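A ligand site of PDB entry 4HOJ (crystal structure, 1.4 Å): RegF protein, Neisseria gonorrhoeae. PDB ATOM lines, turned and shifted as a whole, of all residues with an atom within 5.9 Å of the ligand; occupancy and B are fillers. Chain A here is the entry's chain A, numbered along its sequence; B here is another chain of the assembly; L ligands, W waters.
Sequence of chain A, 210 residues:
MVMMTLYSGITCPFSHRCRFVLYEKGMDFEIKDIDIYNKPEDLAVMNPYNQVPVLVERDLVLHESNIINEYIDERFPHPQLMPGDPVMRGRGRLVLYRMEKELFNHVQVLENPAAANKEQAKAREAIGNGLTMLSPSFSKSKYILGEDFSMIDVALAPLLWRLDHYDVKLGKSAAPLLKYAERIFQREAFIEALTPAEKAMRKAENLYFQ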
ATOM      1  N   THR A  11     -26.101 -15.539  33.927  1.00  0.00           N
ATOM      2  CA  THR A  11     -24.920 -14.736  34.339  1.00  0.00           C
ATOM      3  C   THR A  11     -24.532 -13.728  33.281  1.00  0.00           C
ATOM      4  O   THR A  11     -23.463 -13.130  33.390  1.00  0.00           O
ATOM      5  CB  THR A  11     -23.675 -15.574  34.755  1.00  0.00           C
ATOM      6  OG1 THR A  11     -23.258 -16.362  33.634  1.00  0.00           O
ATOM      7  CG2 THR A  11     -24.016 -16.495  35.939  1.00  0.00           C
ATOM      8  N   CYS A  12     -25.393 -13.487  32.299  1.00  0.00           N
ATOM      9  CA  CYS A  12     -24.999 -12.655  31.168  1.00  0.00           C
ATOM     10  C   CYS A  12     -25.231 -11.176  31.484  1.00  0.00           C
ATOM     11  O   CYS A  12     -26.388 -10.785  31.714  1.00  0.00           O
ATOM     12  CB  CYS A  12     -25.851 -13.068  29.959  1.00  0.00           C
ATOM     13  SG  CYS A  12     -25.668 -12.006  28.526  1.00  0.00           S
ATOM     14  N   PRO A  13     -24.170 -10.352  31.416  1.00  0.00           N
ATOM     15  CA  PRO A  13     -24.385  -8.922  31.745  1.00  0.00           C
ATOM     16  C   PRO A  13     -25.291  -8.227  30.742  1.00  0.00           C
ATOM     17  O   PRO A  13     -25.922  -7.230  31.096  1.00  0.00           O
ATOM     18  CB  PRO A  13     -22.941  -8.333  31.773  1.00  0.00           C
ATOM     19  CG  PRO A  13     -22.099  -9.327  30.906  1.00  0.00           C
ATOM     20  CD  PRO A  13     -22.760 -10.703  31.179  1.00  0.00           C
ATOM     21  N   PHE A  14     -25.320  -8.689  29.493  1.00  0.00           N
ATOM     22  CA  PHE A  14     -26.137  -8.041  28.468  1.00  0.00           C
ATOM     23  C   PHE A  14     -27.571  -8.369  28.669  1.00  0.00           C
ATOM     24  O   PHE A  14     -28.443  -7.489  28.595  1.00  0.00           O
ATOM     25  CB  PHE A  14     -25.631  -8.432  27.064  1.00  0.00           C
ATOM     26  CG  PHE A  14     -24.193  -8.047  26.855  1.00  0.00           C
ATOM     27  CD1 PHE A  14     -23.860  -6.720  26.643  1.00  0.00           C
ATOM     28  CD2 PHE A  14     -23.195  -8.964  26.957  1.00  0.00           C
ATOM     29  CE1 PHE A  14     -22.555  -6.344  26.462  1.00  0.00           C
ATOM     30  CE2 PHE A  14     -21.853  -8.599  26.829  1.00  0.00           C
ATOM     31  CZ  PHE A  14     -21.537  -7.269  26.584  1.00  0.00           C
ATOM     32  N   SER A  15     -27.872  -9.608  29.084  1.00  0.00           N
ATOM     33  CA  SER A  15     -29.231  -9.984  29.499  1.00  0.00           C
ATOM     34  C   SER A  15     -29.680  -9.237  30.774  1.00  0.00           C
ATOM     35  O   SER A  15     -30.843  -8.865  30.920  1.00  0.00           O
ATOM     36  CB  SER A  15     -29.301 -11.527  29.795  1.00  0.00           C
ATOM     37  OG  SER A  15     -29.017 -12.278  28.592  1.00  0.00           O
ATOM     38  N   ARG A  17     -28.938  -6.256  31.557  1.00  0.00           N
ATOM     39  CA  ARG A  17     -29.408  -4.905  31.212  1.00  0.00           C
ATOM     40  C   ARG A  17     -30.886  -4.958  30.894  1.00  0.00           C
ATOM     41  O   ARG A  17     -31.660  -4.086  31.346  1.00  0.00           O
ATOM     42  CB  ARG A  17     -28.709  -4.337  29.942  1.00  0.00           C
ATOM     43  CG  ARG A  17     -27.248  -4.137  30.016  1.00  0.00           C
ATOM     44  CD  ARG A  17     -26.750  -3.718  28.624  1.00  0.00           C
ATOM     45  NE  ARG A  17     -25.398  -3.136  28.674  1.00  0.00           N
ATOM     46  CZ  ARG A  17     -24.706  -2.904  27.557  1.00  0.00           C
ATOM     47  NH1 ARG A  17     -25.119  -3.354  26.356  1.00  0.00           N
ATOM     48  NH2 ARG A  17     -23.549  -2.273  27.709  1.00  0.00           N
ATOM     49  N   ILE A  36     -25.893 -20.801  28.044  1.00  0.00           N
ATOM     50  CA  ILE A  36     -25.064 -20.483  26.897  1.00  0.00           C
ATOM     51  C   ILE A  36     -24.151 -21.655  26.527  1.00  0.00           C
ATOM     52  O   ILE A  36     -23.583 -21.660  25.442  1.00  0.00           O
ATOM     53  CB  ILE A  36     -24.256 -19.201  27.097  1.00  0.00           C
ATOM     54  CG1 ILE A  36     -23.290 -19.342  28.248  1.00  0.00           C
ATOM     55  CG2 ILE A  36     -25.188 -18.018  27.285  1.00  0.00           C
ATOM     56  CD1 ILE A  36     -22.533 -18.040  28.484  1.00  0.00           C
ATOM     57  N   LYS A  39     -27.044 -24.200  24.042  1.00  0.00           N
ATOM     58  CA  LYS A  39     -28.044 -23.335  23.418  1.00  0.00           C
ATOM     59  C   LYS A  39     -29.059 -24.117  22.606  1.00  0.00           C
ATOM     60  O   LYS A  39     -28.721 -25.109  21.948  1.00  0.00           O
ATOM     61  CB  LYS A  39     -27.373 -22.359  22.468  1.00  0.00           C
ATOM     62  CG  LYS A  39     -26.414 -21.466  23.148  1.00  0.00           C
ATOM     63  CD  LYS A  39     -25.558 -20.832  21.994  1.00  0.00           C
ATOM     64  CE  LYS A  39     -24.538 -19.894  22.535  1.00  0.00           C
ATOM     65  NZ  LYS A  39     -23.664 -19.510  21.355  1.00  0.00           N
ATOM     66  N   LEU A  43     -32.304 -20.456  19.084  1.00  0.00           N
ATOM     67  CA  LEU A  43     -31.544 -19.243  19.348  1.00  0.00           C
ATOM     68  C   LEU A  43     -30.886 -18.695  18.077  1.00  0.00           C
ATOM     69  O   LEU A  43     -30.937 -17.474  17.833  1.00  0.00           O
ATOM     70  CB  LEU A  43     -30.508 -19.426  20.466  1.00  0.00           C
ATOM     71  CG  LEU A  43     -29.926 -18.107  20.956  1.00  0.00           C
ATOM     72  CD1 LEU A  43     -30.944 -17.171  21.686  1.00  0.00           C
ATOM     73  CD2 LEU A  43     -28.729 -18.315  21.891  1.00  0.00           C
ATOM     74  N   TYR A  49     -26.309 -14.136  15.391  1.00  0.00           N
ATOM     75  CA  TYR A  49     -25.099 -14.237  16.199  1.00  0.00           C
ATOM     76  C   TYR A  49     -25.161 -15.293  17.297  1.00  0.00           C
ATOM     77  O   TYR A  49     -24.161 -15.516  17.971  1.00  0.00           O
ATOM     78  CB  TYR A  49     -24.754 -12.878  16.816  1.00  0.00           C
ATOM     79  CG  TYR A  49     -24.714 -11.801  15.770  1.00  0.00           C
ATOM     80  CD1 TYR A  49     -23.900 -11.902  14.665  1.00  0.00           C
ATOM     81  CD2 TYR A  49     -25.554 -10.706  15.853  1.00  0.00           C
ATOM     82  CE1 TYR A  49     -23.908 -10.906  13.688  1.00  0.00           C
ATOM     83  CE2 TYR A  49     -25.552  -9.711  14.877  1.00  0.00           C
ATOM     84  CZ  TYR A  49     -24.743  -9.835  13.827  1.00  0.00           C
ATOM     85  OH  TYR A  49     -24.770  -8.807  12.852  1.00  0.00           O
ATOM     86  N   ASN A  50     -26.337 -15.926  17.435  1.00  0.00           N
ATOM     87  CA  ASN A  50     -26.474 -17.064  18.373  1.00  0.00           C
ATOM     88  C   ASN A  50     -26.112 -16.734  19.812  1.00  0.00           C
ATOM     89  O   ASN A  50     -25.358 -17.447  20.479  1.00  0.00           O
ATOM     90  CB  ASN A  50     -25.643 -18.225  17.881  1.00  0.00           C
ATOM     91  CG  ASN A  50     -26.060 -19.549  18.478  1.00  0.00           C
ATOM     92  OD1 ASN A  50     -27.199 -19.725  18.919  1.00  0.00           O
ATOM     93  ND2 ASN A  50     -25.163 -20.517  18.399  1.00  0.00           N
ATOM     94  N   GLN A  51     -26.602 -15.584  20.284  1.00  0.00           N
ATOM     95  CA  GLN A  51     -26.342 -15.040  21.608  1.00  0.00           C
ATOM     96  C   GLN A  51     -27.656 -14.643  22.273  1.00  0.00           C
ATOM     97  O   GLN A  51     -28.688 -14.406  21.646  1.00  0.00           O
ATOM     98  CB  GLN A  51     -25.488 -13.789  21.516  1.00  0.00           C
ATOM     99  CG  GLN A  51     -24.089 -14.076  21.023  1.00  0.00           C
ATOM    100  CD  GLN A  51     -23.256 -12.821  20.952  1.00  0.00           C
ATOM    101  OE1 GLN A  51     -23.782 -11.738  20.654  1.00  0.00           O
ATOM    102  NE2 GLN A  51     -21.966 -12.938  21.249  1.00  0.00           N
ATOM    103  N   VAL A  52     -27.561 -14.556  23.611  1.00  0.00           N
ATOM    104  CA  VAL A  52     -28.566 -13.863  24.404  1.00  0.00           C
ATOM    105  C   VAL A  52     -28.051 -12.460  24.749  1.00  0.00           C
ATOM    106  O   VAL A  52     -26.839 -12.252  24.795  1.00  0.00           O
ATOM    107  CB  VAL A  52     -28.907 -14.642  25.713  1.00  0.00           C
ATOM    108  CG1 VAL A  52     -29.642 -15.891  25.327  1.00  0.00           C
ATOM    109  CG2 VAL A  52     -27.637 -14.921  26.528  1.00  0.00           C
ATOM    110  N   PRO A  53     -28.938 -11.496  24.991  1.00  0.00           N
ATOM    111  CA  PRO A  53     -30.394 -11.657  25.032  1.00  0.00           C
ATOM    112  C   PRO A  53     -31.069 -11.551  23.684  1.00  0.00           C
ATOM    113  O   PRO A  53     -30.546 -10.973  22.686  1.00  0.00           O
ATOM    114  CB  PRO A  53     -30.843 -10.459  25.875  1.00  0.00           C
ATOM    115  CG  PRO A  53     -29.755  -9.381  25.589  1.00  0.00           C
ATOM    116  CD  PRO A  53     -28.474 -10.228  25.559  1.00  0.00           C
ATOM    117  N   HIS A  63     -32.507  -8.704  18.776  1.00  0.00           N
ATOM    118  CA  HIS A  63     -31.348  -8.985  19.602  1.00  0.00           C
ATOM    119  C   HIS A  63     -30.583  -7.660  19.729  1.00  0.00           C
ATOM    120  O   HIS A  63     -31.029  -6.627  19.210  1.00  0.00           O
ATOM    121  CB  HIS A  63     -30.507 -10.115  18.983  1.00  0.00           C
ATOM    122  CG  HIS A  63     -30.158  -9.907  17.534  1.00  0.00           C
ATOM    123  ND1 HIS A  63     -28.986  -9.302  17.100  1.00  0.00           N
ATOM    124  CD2 HIS A  63     -30.821 -10.262  16.407  1.00  0.00           C
ATOM    125  CE1 HIS A  63     -28.983  -9.255  15.773  1.00  0.00           C
ATOM    126  NE2 HIS A  63     -30.090  -9.827  15.323  1.00  0.00           N
ATOM    127  N   GLU A  64     -29.456  -7.741  20.419  1.00  0.00           N
ATOM    128  CA  GLU A  64     -28.599  -6.632  20.822  1.00  0.00           C
ATOM    129  C   GLU A  64     -29.239  -5.865  21.958  1.00  0.00           C
ATOM    130  O   GLU A  64     -30.235  -5.127  21.815  1.00  0.00           O
ATOM    131  CB  GLU A  64     -28.326  -5.694  19.628  1.00  0.00           C
ATOM    132  CG  GLU A  64     -27.245  -4.659  19.909  1.00  0.00           C
ATOM    133  CD  GLU A  64     -25.876  -5.224  20.157  1.00  0.00           C
ATOM    134  OE1 GLU A  64     -25.645  -6.418  19.938  1.00  0.00           O
ATOM    135  OE2 GLU A  64     -24.998  -4.377  20.485  1.00  0.00           O
ATOM    136  N   SER A  65     -28.681  -6.079  23.154  1.00  0.00           N
ATOM    137  CA  SER A  65     -29.270  -5.564  24.396  1.00  0.00           C
ATOM    138  C   SER A  65     -29.662  -4.094  24.358  1.00  0.00           C
ATOM    139  O   SER A  65     -30.796  -3.781  24.797  1.00  0.00           O
ATOM    140  CB  SER A  65     -28.336  -5.889  25.576  1.00  0.00           C
ATOM    141  OG  SER A  65     -27.070  -5.228  25.468  1.00  0.00           O
ATOM    142  N   ASN A  66     -28.811  -3.227  23.812  1.00  0.00           N
ATOM    143  CA  ASN A  66     -29.201  -1.813  23.880  1.00  0.00           C
ATOM    144  C   ASN A  66     -30.351  -1.491  22.931  1.00  0.00           C
ATOM    145  O   ASN A  66     -31.120  -0.584  23.170  1.00  0.00           O
ATOM    146  CB  ASN A  66     -28.010  -0.911  23.540  1.00  0.00           C
ATOM    147  CG  ASN A  66     -27.028  -0.794  24.670  1.00  0.00           C
ATOM    148  OD1 ASN A  66     -27.295  -1.116  25.817  1.00  0.00           O
ATOM    149  ND2 ASN A  66     -25.838  -0.328  24.310  1.00  0.00           N
ATOM    150  N   GLU A 100     -19.975   0.819  24.578  1.00  0.00           N
ATOM    151  CA  GLU A 100     -19.948  -0.442  23.859  1.00  0.00           C
ATOM    152  C   GLU A 100     -18.611  -0.668  23.277  1.00  0.00           C
ATOM    153  O   GLU A 100     -18.089  -1.802  23.282  1.00  0.00           O
ATOM    154  CB  GLU A 100     -21.032  -0.584  22.743  1.00  0.00           C
ATOM    155  CG  GLU A 100     -22.489  -0.970  23.113  1.00  0.00           C
ATOM    156  CD  GLU A 100     -22.766  -1.979  24.321  1.00  0.00           C
ATOM    157  OE1 GLU A 100     -23.349  -3.094  24.199  1.00  0.00           O
ATOM    158  OE2 GLU A 100     -22.435  -1.544  25.356  1.00  0.00           O
ATOM    159  N   GLN A 108     -16.893  -8.533  26.810  1.00  0.00           N
ATOM    160  CA  GLN A 108     -17.060  -9.756  26.014  1.00  0.00           C
ATOM    161  C   GLN A 108     -15.879 -10.691  26.069  1.00  0.00           C
ATOM    162  O   GLN A 108     -16.050 -11.925  25.997  1.00  0.00           O
ATOM    163  CB  GLN A 108     -17.383  -9.400  24.539  1.00  0.00           C
ATOM    164  CG  GLN A 108     -18.774  -8.713  24.416  1.00  0.00           C
ATOM    165  CD  GLN A 108     -19.127  -8.302  22.994  1.00  0.00           C
ATOM    166  OE1 GLN A 108     -19.199  -9.155  22.110  1.00  0.00           O
ATOM    167  NE2 GLN A 108     -19.256  -7.008  22.762  1.00  0.00           N
ATOM    168  N   GLU A 111     -16.029 -12.551  29.247  1.00  0.00           N
ATOM    169  CA  GLU A 111     -17.111 -13.530  29.195  1.00  0.00           C
ATOM    170  C   GLU A 111     -16.857 -14.723  28.272  1.00  0.00           C
ATOM    171  O   GLU A 111     -17.604 -15.710  28.321  1.00  0.00           O
ATOM    172  CB  GLU A 111     -18.432 -12.851  28.749  1.00  0.00           C
ATOM    173  CG  GLU A 111     -19.076 -11.871  29.790  1.00  0.00           C
ATOM    174  CD  GLU A 111     -19.590 -12.618  31.011  1.00  0.00           C
ATOM    175  OE1 GLU A 111     -20.113 -13.714  30.891  1.00  0.00           O
ATOM    176  OE2 GLU A 111     -19.426 -12.058  32.095  1.00  0.00           O
ATOM    177  N   TYR B  97     -27.956  -1.646  12.903  1.00  0.00           N
ATOM    178  CA  TYR B  97     -26.880  -2.275  13.632  1.00  0.00           C
ATOM    179  C   TYR B  97     -26.275  -3.388  12.783  1.00  0.00           C
ATOM    180  O   TYR B  97     -25.031  -3.501  12.686  1.00  0.00           O
ATOM    181  CB  TYR B  97     -27.452  -2.835  14.981  1.00  0.00           C
ATOM    182  CG  TYR B  97     -26.387  -3.636  15.734  1.00  0.00           C
ATOM    183  CD1 TYR B  97     -25.439  -3.004  16.544  1.00  0.00           C
ATOM    184  CD2 TYR B  97     -26.321  -4.985  15.634  1.00  0.00           C
ATOM    185  CE1 TYR B  97     -24.423  -3.719  17.199  1.00  0.00           C
ATOM    186  CE2 TYR B  97     -25.318  -5.729  16.308  1.00  0.00           C
ATOM    187  CZ  TYR B  97     -24.356  -5.079  17.050  1.00  0.00           C
ATOM    188  OH  TYR B  97     -23.345  -5.756  17.666  1.00  0.00           O
HETATM  189  N1  LIG L   1     -23.719  -7.261  21.691  1.00  0.00           N
HETATM  190  C1  LIG L   1     -24.529  -8.251  22.450  1.00  0.00           C
HETATM  191  C2  LIG L   1     -25.603  -7.565  23.212  1.00  0.00           C
HETATM  192  O1  LIG L   1     -26.698  -8.137  23.405  1.00  0.00           O
HETATM  193  O2  LIG L   1     -25.339  -6.437  23.661  1.00  0.00           O
HETATM  194  C3  LIG L   1     -23.646  -9.165  23.304  1.00  0.00           C
HETATM  195  C4  LIG L   1     -24.397 -10.358  23.896  1.00  0.00           C
HETATM  196  C5  LIG L   1     -23.410 -11.395  24.414  1.00  0.00           C
HETATM  197  O3  LIG L   1     -22.208 -11.252  24.410  1.00  0.00           O
HETATM  198  N2  LIG L   1     -24.053 -12.489  24.970  1.00  0.00           N
HETATM  199  C6  LIG L   1     -23.239 -13.583  25.482  1.00  0.00           C
HETATM  200  C7  LIG L   1     -23.585 -14.803  24.662  1.00  0.00           C
HETATM  201  O4  LIG L   1     -24.692 -15.138  24.268  1.00  0.00           O
HETATM  202  C8  LIG L   1     -23.485 -13.956  26.904  1.00  0.00           C
HETATM  203  S1  LIG L   1     -23.263 -12.618  28.045  1.00  0.00           S
HETATM  204  N3  LIG L   1     -22.455 -15.685  24.442  1.00  0.00           N
HETATM  205  C9  LIG L   1     -22.602 -16.904  23.660  1.00  0.00           C
HETATM  206  C10 LIG L   1     -21.720 -16.773  22.462  1.00  0.00           C
HETATM  207  O5  LIG L   1     -21.109 -15.710  22.087  1.00  0.00           O
HETATM  208  O6  LIG L   1     -21.623 -17.820  21.772  1.00  0.00           O
HETATM  209  O   HOH W   1     -19.899 -11.424  22.573  1.00  0.00           O
HETATM  210  O   HOH W   2     -25.977  -3.499  23.008  1.00  0.00           O
HETATM  211  O   HOH W   3     -22.292  -5.239  23.087  1.00  0.00           O
HETATM  212  O   HOH W   4     -22.258 -17.367  19.388  1.00  0.00           O
HETATM  213  O   HOH W   5     -28.145  -9.938  21.871  1.00  0.00           O
HETATM  214  O   HOH W   6     -20.216 -11.575  26.342  1.00  0.00           O
HETATM  215  O   HOH W   7     -20.170 -14.945  26.124  1.00  0.00           O
HETATM  216  O   HOH W   8     -19.977 -15.011  19.234  1.00  0.00           O
HETATM  217  O   HOH W   9     -22.471  -9.296  20.021  1.00  0.00           O
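The side-chain hydroxyl (OG) of Ser 65 is in hydrogen-bond range of an oxygen (O2) of the ligand, at 2.8 Å. The backbone carbonyl oxygen (O) of Val 52 lies within hydrogen-bond range of a nitrogen (N2) of the ligand, at 2.8 Å. The side-chain carboxylate (OE1) of Glu 64 lies within salt-bridge range of a nitrogen (N1) of the ligand (2.7 Å). The backbone NH of Ser 65 is in hydrogen-bond range of an oxygen (O1) of the ligand (2.9 Å). NE2 of Gln 51 sits at hydrogen-bond distance from O5 of the ligand. N of Val 52 lies within hydrogen-bond range of O4 of the ligand, 3.0 Å away. NZ of Lys 39 lies within salt-bridge range of O6 of the ligand (2.7 Å). The side-chain sulfur (SG) of Cys 12 sits close to a sulfur (S1) of the ligand (2.5 Å).
The backbone NH of Ser 15 lies within hydrogen-bond range of the side-chain sulfur of Cys 12 (3.3 Å). The side-chain carboxylate (OE1) of Glu 64 is in hydrogen-bond range of the side-chain hydroxyl (OH) of Tyr 97 of chain B (3.3 Å). The side-chain sulfur of Cys 12 sits close to the backbone NH of Phe 14 (3.5 Å). NH2 of Arg 17 lies within salt-bridge range of OE2 of Glu 100 (2.7 Å). The side-chain hydroxyl of Ser 65 sits at hydrogen-bond distance from the guanidinium group of Arg 17. NZ of Lys 39 is in hydrogen-bond range of O of Asn 50, at 2.8 Å.
Residues that only touch the ligand: Pro 13 (3.7 Å), Phe 14 (3.3 Å), Asn 50 (3.97 Å), Pro 53 (3.5 Å) and Glu 100 (3.9 Å). Hydrophobic or aromatic side chains that line the ligand: Pro 13, Phe 14, Val 52 and Pro 53. Of the 22 residues printed, 11 come within 4 Å of the ligand. The nearest printed residue that does not touch the ligand is Arg 17 (4.1 Å).
Water W4 lies within hydrogen-bond range of O6 of the ligand, O of Tyr 49, NZ of Lys 39 and O of Asn 50. Water W5 lies within hydrogen-bond range of O of Pro 53 (2.7 Å), O1 of the ligand (2.8 Å) and N of Glu 64 (2.9 Å). Water W9 bridges the side-chain amide oxygen of Gln 51 (2.8 Å) and a nitrogen (N1) of the ligand (2.9 Å). Water W7 lies within hydrogen-bond range of N3 of the ligand (2.9 Å) and O of Glu 111 (3.5 Å). Water W1 lies within hydrogen-bond range of the side-chain amide oxygen (OE1) of Gln 108 (2.4 Å), the side-chain amide nitrogen (NE2) of Gln 51 (2.9 Å) and an oxygen (O3) of the ligand (3.0 Å). Water W2 lies within hydrogen-bond range of OE2 of Glu 64, OE1 of Glu 100, N of Asn 66, O2 of the ligand, OG of Ser 65 and NH1 of Arg 17.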
